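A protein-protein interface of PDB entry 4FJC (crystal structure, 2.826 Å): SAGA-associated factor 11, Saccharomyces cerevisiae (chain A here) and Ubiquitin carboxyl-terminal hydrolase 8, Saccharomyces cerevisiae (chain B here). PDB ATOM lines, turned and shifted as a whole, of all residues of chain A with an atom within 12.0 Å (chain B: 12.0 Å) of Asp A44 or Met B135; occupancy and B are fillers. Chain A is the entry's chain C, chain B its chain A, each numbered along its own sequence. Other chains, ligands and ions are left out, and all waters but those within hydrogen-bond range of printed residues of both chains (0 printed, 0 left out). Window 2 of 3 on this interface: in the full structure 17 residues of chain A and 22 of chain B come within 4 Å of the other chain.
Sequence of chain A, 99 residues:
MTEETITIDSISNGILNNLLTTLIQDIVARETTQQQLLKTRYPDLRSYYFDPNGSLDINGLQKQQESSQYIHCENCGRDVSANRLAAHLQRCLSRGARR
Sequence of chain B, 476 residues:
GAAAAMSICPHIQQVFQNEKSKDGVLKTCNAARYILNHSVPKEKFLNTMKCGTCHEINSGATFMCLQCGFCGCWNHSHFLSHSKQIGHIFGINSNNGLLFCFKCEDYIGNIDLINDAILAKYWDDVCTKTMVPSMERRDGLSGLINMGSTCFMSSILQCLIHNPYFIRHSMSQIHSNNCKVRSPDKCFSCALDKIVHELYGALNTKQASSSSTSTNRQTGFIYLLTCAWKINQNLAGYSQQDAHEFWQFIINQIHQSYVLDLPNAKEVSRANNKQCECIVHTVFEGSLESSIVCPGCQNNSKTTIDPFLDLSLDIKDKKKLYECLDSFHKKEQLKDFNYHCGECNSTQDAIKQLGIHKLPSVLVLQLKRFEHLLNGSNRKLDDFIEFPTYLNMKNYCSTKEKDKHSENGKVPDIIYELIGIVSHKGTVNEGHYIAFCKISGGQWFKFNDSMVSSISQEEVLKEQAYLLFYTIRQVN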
ATOM      1  N   GLN A  34      11.058  -1.493  37.871  1.00  0.00           N
ATOM      2  CA  GLN A  34      10.881  -2.383  36.761  1.00  0.00           C
ATOM      3  C   GLN A  34       9.411  -2.327  36.339  1.00  0.00           C
ATOM      4  O   GLN A  34       9.091  -2.474  35.159  1.00  0.00           O
ATOM      5  CB  GLN A  34      11.304  -3.773  37.234  1.00  0.00           C
ATOM      6  CG  GLN A  34      11.416  -4.879  36.208  1.00  0.00           C
ATOM      7  CD  GLN A  34      11.339  -6.260  36.855  1.00  0.00           C
ATOM      8  OE1 GLN A  34      12.029  -6.530  37.848  1.00  0.00           O
ATOM      9  NE2 GLN A  34      10.489  -7.133  36.308  1.00  0.00           N
ATOM     10  N   GLN A  35       8.522  -2.113  37.311  1.00  0.00           N
ATOM     11  CA  GLN A  35       7.077  -2.134  37.090  1.00  0.00           C
ATOM     12  C   GLN A  35       6.591  -0.757  36.622  1.00  0.00           C
ATOM     13  O   GLN A  35       5.692  -0.662  35.802  1.00  0.00           O
ATOM     14  CB  GLN A  35       6.384  -2.555  38.397  1.00  0.00           C
ATOM     15  CG  GLN A  35       4.872  -2.627  38.375  1.00  0.00           C
ATOM     16  CD  GLN A  35       4.336  -3.606  37.348  1.00  0.00           C
ATOM     17  OE1 GLN A  35       5.068  -4.445  36.806  1.00  0.00           O
ATOM     18  NE2 GLN A  35       3.045  -3.511  37.084  1.00  0.00           N
ATOM     19  N   GLN A  36       7.183   0.305  37.153  1.00  0.00           N
ATOM     20  CA  GLN A  36       6.965   1.643  36.629  1.00  0.00           C
ATOM     21  C   GLN A  36       7.249   1.648  35.122  1.00  0.00           C
ATOM     22  O   GLN A  36       6.431   2.100  34.340  1.00  0.00           O
ATOM     23  CB  GLN A  36       7.852   2.671  37.372  1.00  0.00           C
ATOM     24  CG  GLN A  36       7.580   4.114  37.014  1.00  0.00           C
ATOM     25  CD  GLN A  36       8.619   5.097  37.559  1.00  0.00           C
ATOM     26  OE1 GLN A  36       9.801   4.971  37.288  1.00  0.00           O
ATOM     27  NE2 GLN A  36       8.167   6.116  38.271  1.00  0.00           N
ATOM     28  N   LEU A  37       8.413   1.135  34.733  1.00  0.00           N
ATOM     29  CA  LEU A  37       8.814   1.061  33.340  1.00  0.00           C
ATOM     30  C   LEU A  37       7.774   0.350  32.497  1.00  0.00           C
ATOM     31  O   LEU A  37       7.424   0.860  31.456  1.00  0.00           O
ATOM     32  CB  LEU A  37      10.150   0.328  33.182  1.00  0.00           C
ATOM     33  CG  LEU A  37      10.611   0.132  31.722  1.00  0.00           C
ATOM     34  CD1 LEU A  37      10.802   1.512  31.119  1.00  0.00           C
ATOM     35  CD2 LEU A  37      11.879  -0.692  31.544  1.00  0.00           C
ATOM     36  N   LEU A  38       7.295  -0.819  32.922  1.00  0.00           N
ATOM     37  CA  LEU A  38       6.309  -1.566  32.134  1.00  0.00           C
ATOM     38  C   LEU A  38       4.963  -0.852  31.969  1.00  0.00           C
ATOM     39  O   LEU A  38       4.332  -1.003  30.940  1.00  0.00           O
ATOM     40  CB  LEU A  38       6.099  -2.991  32.681  1.00  0.00           C
ATOM     41  CG  LEU A  38       7.177  -3.965  32.160  1.00  0.00           C
ATOM     42  CD1 LEU A  38       7.752  -4.918  33.230  1.00  0.00           C
ATOM     43  CD2 LEU A  38       6.692  -4.717  30.925  1.00  0.00           C
ATOM     44  N   LYS A  39       4.548  -0.067  32.959  1.00  0.00           N
ATOM     45  CA  LYS A  39       3.287   0.673  32.905  1.00  0.00           C
ATOM     46  C   LYS A  39       3.359   1.932  32.026  1.00  0.00           C
ATOM     47  O   LYS A  39       2.410   2.266  31.330  1.00  0.00           O
ATOM     48  CB  LYS A  39       2.805   1.025  34.329  1.00  0.00           C
ATOM     49  CG  LYS A  39       2.110  -0.146  35.042  1.00  0.00           C
ATOM     50  CD  LYS A  39       1.636   0.148  36.473  1.00  0.00           C
ATOM     51  CE  LYS A  39       0.131   0.402  36.572  1.00  0.00           C
ATOM     52  NZ  LYS A  39      -0.747  -0.479  35.704  1.00  0.00           N
ATOM     53  N   THR A  40       4.478   2.631  32.080  1.00  0.00           N
ATOM     54  CA  THR A  40       4.763   3.750  31.177  1.00  0.00           C
ATOM     55  C   THR A  40       4.952   3.276  29.730  1.00  0.00           C
ATOM     56  O   THR A  40       4.602   3.958  28.785  1.00  0.00           O
ATOM     57  CB  THR A  40       6.064   4.450  31.614  1.00  0.00           C
ATOM     58  OG1 THR A  40       6.191   4.364  33.037  1.00  0.00           O
ATOM     59  CG2 THR A  40       6.093   5.895  31.200  1.00  0.00           C
ATOM     60  N   ARG A  41       5.523   2.101  29.563  1.00  0.00           N
ATOM     61  CA  ARG A  41       5.842   1.609  28.249  1.00  0.00           C
ATOM     62  C   ARG A  41       4.634   0.982  27.540  1.00  0.00           C
ATOM     63  O   ARG A  41       4.540   1.005  26.307  1.00  0.00           O
ATOM     64  CB  ARG A  41       6.953   0.586  28.378  1.00  0.00           C
ATOM     65  CG  ARG A  41       7.552   0.158  27.061  1.00  0.00           C
ATOM     66  CD  ARG A  41       8.736  -0.747  27.275  1.00  0.00           C
ATOM     67  NE  ARG A  41       9.970  -0.001  27.534  1.00  0.00           N
ATOM     68  CZ  ARG A  41      11.179  -0.510  27.377  1.00  0.00           C
ATOM     69  NH1 ARG A  41      11.332  -1.746  26.977  1.00  0.00           N
ATOM     70  NH2 ARG A  41      12.226   0.223  27.592  1.00  0.00           N
ATOM     71  N   TYR A  42       3.733   0.409  28.335  1.00  0.00           N
ATOM     72  CA  TYR A  42       2.583  -0.332  27.854  1.00  0.00           C
ATOM     73  C   TYR A  42       1.352  -0.014  28.707  1.00  0.00           C
ATOM     74  O   TYR A  42       1.025  -0.797  29.613  1.00  0.00           O
ATOM     75  CB  TYR A  42       2.868  -1.825  27.951  1.00  0.00           C
ATOM     76  CG  TYR A  42       4.144  -2.273  27.276  1.00  0.00           C
ATOM     77  CD1 TYR A  42       4.403  -1.959  25.946  1.00  0.00           C
ATOM     78  CD2 TYR A  42       5.087  -3.034  27.966  1.00  0.00           C
ATOM     79  CE1 TYR A  42       5.576  -2.364  25.326  1.00  0.00           C
ATOM     80  CE2 TYR A  42       6.257  -3.447  27.353  1.00  0.00           C
ATOM     81  CZ  TYR A  42       6.498  -3.104  26.035  1.00  0.00           C
ATOM     82  OH  TYR A  42       7.657  -3.525  25.430  1.00  0.00           O
ATOM     83  N   PRO A  43       0.687   1.150  28.452  1.00  0.00           N
ATOM     84  CA  PRO A  43      -0.560   1.570  29.145  1.00  0.00           C
ATOM     85  C   PRO A  43      -1.662   0.523  29.087  1.00  0.00           C
ATOM     86  O   PRO A  43      -2.436   0.384  30.030  1.00  0.00           O
ATOM     87  CB  PRO A  43      -1.003   2.813  28.388  1.00  0.00           C
ATOM     88  CG  PRO A  43       0.125   3.201  27.492  1.00  0.00           C
ATOM     89  CD  PRO A  43       1.275   2.261  27.680  1.00  0.00           C
ATOM     90  N   ASP A  44      -1.728  -0.202  27.981  1.00  0.00           N
ATOM     91  CA  ASP A  44      -2.558  -1.398  27.915  1.00  0.00           C
ATOM     92  C   ASP A  44      -1.735  -2.575  28.439  1.00  0.00           C
ATOM     93  O   ASP A  44      -0.508  -2.600  28.302  1.00  0.00           O
ATOM     94  CB  ASP A  44      -3.012  -1.628  26.477  1.00  0.00           C
ATOM     95  CG  ASP A  44      -3.516  -0.350  25.832  1.00  0.00           C
ATOM     96  OD1 ASP A  44      -4.532   0.182  26.331  1.00  0.00           O
ATOM     97  OD2 ASP A  44      -2.885   0.141  24.861  1.00  0.00           O
ATOM     98  N   LEU A  45      -2.403  -3.548  29.041  1.00  0.00           N
ATOM     99  CA  LEU A  45      -1.710  -4.654  29.687  1.00  0.00           C
ATOM    100  C   LEU A  45      -2.666  -5.807  29.967  1.00  0.00           C
ATOM    101  O   LEU A  45      -2.364  -6.688  30.767  1.00  0.00           O
ATOM    102  CB  LEU A  45      -1.069  -4.160  30.986  1.00  0.00           C
ATOM    103  CG  LEU A  45      -2.029  -3.473  31.977  1.00  0.00           C
ATOM    104  CD1 LEU A  45      -2.589  -4.457  33.014  1.00  0.00           C
ATOM    105  CD2 LEU A  45      -1.339  -2.274  32.632  1.00  0.00           C
ATOM    106  N   ALA B   5      -2.548   7.870  33.205  1.00  0.00           N
ATOM    107  CA  ALA B   5      -1.202   7.552  32.658  1.00  0.00           C
ATOM    108  C   ALA B   5      -0.120   7.675  33.737  1.00  0.00           C
ATOM    109  O   ALA B   5      -0.271   8.435  34.699  1.00  0.00           O
ATOM    110  CB  ALA B   5      -0.878   8.461  31.475  1.00  0.00           C
ATOM    111  N   MET B   6       0.965   6.909  33.576  1.00  0.00           N
ATOM    112  CA  MET B   6       2.155   7.068  34.415  1.00  0.00           C
ATOM    113  C   MET B   6       2.785   8.429  34.153  1.00  0.00           C
ATOM    114  O   MET B   6       2.630   9.001  33.073  1.00  0.00           O
ATOM    115  CB  MET B   6       3.191   5.980  34.138  1.00  0.00           C
ATOM    116  CG  MET B   6       2.820   4.609  34.668  1.00  0.00           C
ATOM    117  SD  MET B   6       2.906   4.439  36.467  1.00  0.00           S
ATOM    118  CE  MET B   6       1.200   4.760  36.927  1.00  0.00           C
ATOM    119  N   MET B 131      13.451   0.794  18.211  1.00  0.00           N
ATOM    120  CA  MET B 131      12.229   0.973  18.997  1.00  0.00           C
ATOM    121  C   MET B 131      12.173   0.000  20.200  1.00  0.00           C
ATOM    122  O   MET B 131      12.831  -1.059  20.216  1.00  0.00           O
ATOM    123  CB  MET B 131      11.000   0.840  18.067  1.00  0.00           C
ATOM    124  CG  MET B 131      10.412  -0.564  17.898  1.00  0.00           C
ATOM    125  SD  MET B 131       9.705  -1.031  16.281  1.00  0.00           S
ATOM    126  CE  MET B 131       9.060   0.560  15.744  1.00  0.00           C
ATOM    127  N   VAL B 132      11.398   0.348  21.230  1.00  0.00           N
ATOM    128  CA  VAL B 132      11.265  -0.552  22.376  1.00  0.00           C
ATOM    129  C   VAL B 132      10.508  -1.791  21.904  1.00  0.00           C
ATOM    130  O   VAL B 132       9.801  -1.725  20.929  1.00  0.00           O
ATOM    131  CB  VAL B 132      10.578   0.099  23.605  1.00  0.00           C
ATOM    132  CG1 VAL B 132      11.286   1.388  23.989  1.00  0.00           C
ATOM    133  CG2 VAL B 132       9.095   0.302  23.400  1.00  0.00           C
ATOM    134  N   PRO B 133      10.665  -2.934  22.592  1.00  0.00           N
ATOM    135  CA  PRO B 133       9.948  -4.119  22.136  1.00  0.00           C
ATOM    136  C   PRO B 133       8.430  -4.015  22.274  1.00  0.00           C
ATOM    137  O   PRO B 133       7.926  -3.396  23.184  1.00  0.00           O
ATOM    138  CB  PRO B 133      10.482  -5.223  23.050  1.00  0.00           C
ATOM    139  CG  PRO B 133      11.771  -4.673  23.592  1.00  0.00           C
ATOM    140  CD  PRO B 133      11.477  -3.231  23.786  1.00  0.00           C
ATOM    141  N   SER B 134       7.720  -4.644  21.350  1.00  0.00           N
ATOM    142  CA  SER B 134       6.274  -4.722  21.402  1.00  0.00           C
ATOM    143  C   SER B 134       5.804  -5.543  22.606  1.00  0.00           C
ATOM    144  O   SER B 134       6.422  -6.547  22.989  1.00  0.00           O
ATOM    145  CB  SER B 134       5.746  -5.343  20.109  1.00  0.00           C
ATOM    146  OG  SER B 134       6.284  -6.651  19.949  1.00  0.00           O
ATOM    147  N   MET B 135       4.688  -5.114  23.182  1.00  0.00           N
ATOM    148  CA  MET B 135       4.123  -5.775  24.353  1.00  0.00           C
ATOM    149  C   MET B 135       4.119  -7.299  24.226  1.00  0.00           C
ATOM    150  O   MET B 135       4.486  -7.989  25.164  1.00  0.00           O
ATOM    151  CB  MET B 135       2.704  -5.272  24.608  1.00  0.00           C
ATOM    152  CG  MET B 135       2.139  -5.644  25.972  1.00  0.00           C
ATOM    153  SD  MET B 135       0.392  -5.188  26.097  1.00  0.00           S
ATOM    154  CE  MET B 135       0.463  -3.425  25.718  1.00  0.00           C
ATOM    155  N   GLU B 136       3.757  -7.804  23.048  1.00  0.00           N
ATOM    156  CA  GLU B 136       3.479  -9.225  22.857  1.00  0.00           C
ATOM    157  C   GLU B 136       4.763 -10.031  22.565  1.00  0.00           C
ATOM    158  O   GLU B 136       4.807 -11.258  22.734  1.00  0.00           O
ATOM    159  CB  GLU B 136       2.460  -9.429  21.718  1.00  0.00           C
ATOM    160  CG  GLU B 136       1.398  -8.323  21.462  1.00  0.00           C
ATOM    161  CD  GLU B 136       1.892  -7.129  20.621  1.00  0.00           C
ATOM    162  OE1 GLU B 136       1.685  -5.989  21.087  1.00  0.00           O
ATOM    163  OE2 GLU B 136       2.470  -7.296  19.507  1.00  0.00           O
ATOM    164  N   ARG B 137       5.818  -9.368  22.104  1.00  0.00           N
ATOM    165  CA  ARG B 137       7.075 -10.089  21.845  1.00  0.00           C
ATOM    166  C   ARG B 137       8.123  -9.944  22.957  1.00  0.00           C
ATOM    167  O   ARG B 137       9.121 -10.647  22.940  1.00  0.00           O
ATOM    168  CB  ARG B 137       7.691  -9.653  20.518  1.00  0.00           C
ATOM    169  CG  ARG B 137       6.794  -9.765  19.305  1.00  0.00           C
ATOM    170  CD  ARG B 137       6.822 -11.147  18.654  1.00  0.00           C
ATOM    171  NE  ARG B 137       5.641 -11.907  19.047  1.00  0.00           N
ATOM    172  CZ  ARG B 137       5.554 -12.754  20.065  1.00  0.00           C
ATOM    173  NH1 ARG B 137       6.576 -13.034  20.858  1.00  0.00           N
ATOM    174  NH2 ARG B 137       4.407 -13.350  20.286  1.00  0.00           N
ATOM    175  N   ARG B 138       7.892  -9.050  23.915  1.00  0.00           N
ATOM    176  CA  ARG B 138       8.940  -8.650  24.853  1.00  0.00           C
ATOM    177  C   ARG B 138       9.592  -9.786  25.612  1.00  0.00           C
ATOM    178  O   ARG B 138      10.749  -9.684  25.973  1.00  0.00           O
ATOM    179  CB  ARG B 138       8.413  -7.645  25.866  1.00  0.00           C
ATOM    180  CG  ARG B 138       7.714  -8.241  27.072  1.00  0.00           C
ATOM    181  CD  ARG B 138       7.209  -7.124  27.973  1.00  0.00           C
ATOM    182  NE  ARG B 138       6.278  -7.602  28.989  1.00  0.00           N
ATOM    183  CZ  ARG B 138       5.007  -7.904  28.749  1.00  0.00           C
ATOM    184  NH1 ARG B 138       4.483  -7.770  27.529  1.00  0.00           N
ATOM    185  NH2 ARG B 138       4.244  -8.346  29.728  1.00  0.00           N
ATOM    186  N   ASP B 139       8.863 -10.856  25.887  1.00  0.00           N
ATOM    187  CA  ASP B 139       9.442 -11.967  26.614  1.00  0.00           C
ATOM    188  C   ASP B 139       9.764 -13.177  25.721  1.00  0.00           C
ATOM    189  O   ASP B 139      10.131 -14.217  26.213  1.00  0.00           O
ATOM    190  CB  ASP B 139       8.541 -12.319  27.802  1.00  0.00           C
ATOM    191  CG  ASP B 139       8.534 -11.206  28.888  1.00  0.00           C
ATOM    192  OD1 ASP B 139       9.635 -10.702  29.244  1.00  0.00           O
ATOM    193  OD2 ASP B 139       7.439 -10.825  29.383  1.00  0.00           O
ATOM    194  N   GLY B 140       9.668 -13.025  24.404  1.00  0.00           N
ATOM    195  CA  GLY B 140       9.976 -14.095  23.456  1.00  0.00           C
ATOM    196  C   GLY B 140       9.008 -15.250  23.417  1.00  0.00           C
ATOM    197  O   GLY B 140       9.357 -16.315  22.905  1.00  0.00           O
ATOM    198  N   LEU B 141       7.797 -15.033  23.941  1.00  0.00           N
ATOM    199  CA  LEU B 141       6.805 -16.096  24.160  1.00  0.00           C
ATOM    200  C   LEU B 141       6.006 -16.396  22.934  1.00  0.00           C
ATOM    201  O   LEU B 141       5.386 -15.497  22.385  1.00  0.00           O
ATOM    202  CB  LEU B 141       5.831 -15.707  25.267  1.00  0.00           C
ATOM    203  CG  LEU B 141       6.439 -15.687  26.675  1.00  0.00           C
ATOM    204  CD1 LEU B 141       5.399 -15.414  27.765  1.00  0.00           C
ATOM    205  CD2 LEU B 141       7.210 -16.977  26.961  1.00  0.00           C
ATOM    206  N   SER B 142       5.991 -17.662  22.526  1.00  0.00           N
ATOM    207  CA  SER B 142       5.321 -18.110  21.287  1.00  0.00           C
ATOM    208  C   SER B 142       5.468 -19.637  21.058  1.00  0.00           C
ATOM    209  O   SER B 142       6.516 -20.240  21.372  1.00  0.00           O
ATOM    210  CB  SER B 142       5.873 -17.348  20.063  1.00  0.00           C
ATOM    211  OG  SER B 142       5.743 -18.088  18.852  1.00  0.00           O
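O of Pro B133 lies close to OH of Tyr A42. O of Asp A44 sits close to SD of Met B135.
Of the 12 printed residues of chain A, 6 touch a printed residue of chain B. Printed residues of chain B that touch a printed residue of chain A: Met B6, Val B132, Pro B133, Ser B134, Met B135 and Arg B138. Hydrophobic or aromatic side chains of chain B within 4 Å of the printed part of chain A: Met B6, Val B132, Pro B133 and Met B135. Among the printed residues, no Asp or Glu carboxylate lies within 4 Å of a Lys or Arg side-chain nitrogen of the other chain.
The backbone NH (N) of Arg B137 lies close to the side-chain hydroxyl (OG) of Ser B134 (3.5 Å). OD2 of Asp B139 lies within salt-bridge range of NE of Arg B138 (3.4 Å). OG1 of Thr A40 sits at hydrogen-bond distance from O of Gln A36 (2.6 Å).
Leu A38 touches Arg B138. Lys A39 touches Met B6 (CB to CG, 3.6 Å). Thr A40 touches Met B6 (OG1 to CB, 3.6 Å). Arg A41 touches Val B132 (CZ to CB, 3.9 Å). NH1 of Arg A41 touches CD of Pro B133, 3.5 Å away. Tyr A42 touches Ser B134. N of Met B135 touches CE1 of Tyr A42 (3.6 Å). CD of Arg B138 touches CE2 of Tyr A42 (3.8 Å).
Printed residues of chain B within 4 Å of Asp A44: Met B135. Met B135 touches just these residues of chain A: Tyr A42 (3.6 Å) and Asp A44 (2.9 Å). Of the printed residues of chain B, Tyr A42 touches Pro B133 (2.3 Å), Ser B134 (3.9 Å), Met B135 (3.6 Å) and Arg B138 (3.8 Å). Ser B134 touches one residue of chain A. No residue of chain A comes within 4 Å of Glu B136. Of the printed residues of chain A, Val B132 touches Arg A41 (3.9 Å). Of the printed residues of chain B, Thr A40 touches Met B6 (3.6 Å). Of the printed residues of chain B, Arg A41 touches Val B132 (3.9 Å) and Pro B133 (3.5 Å). Of the printed residues of chain A, Met B6 touches Lys A39 and Thr A40. Printed residues of chain B within 4 Å of Leu A38: Arg B138. Leu A37 touches none of the printed residues of chain B. Ala B5 touches none of the printed residues of chain A. The nearest residue of chain B that does not touch Asp A44 is Arg B138 (7.2 Å).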
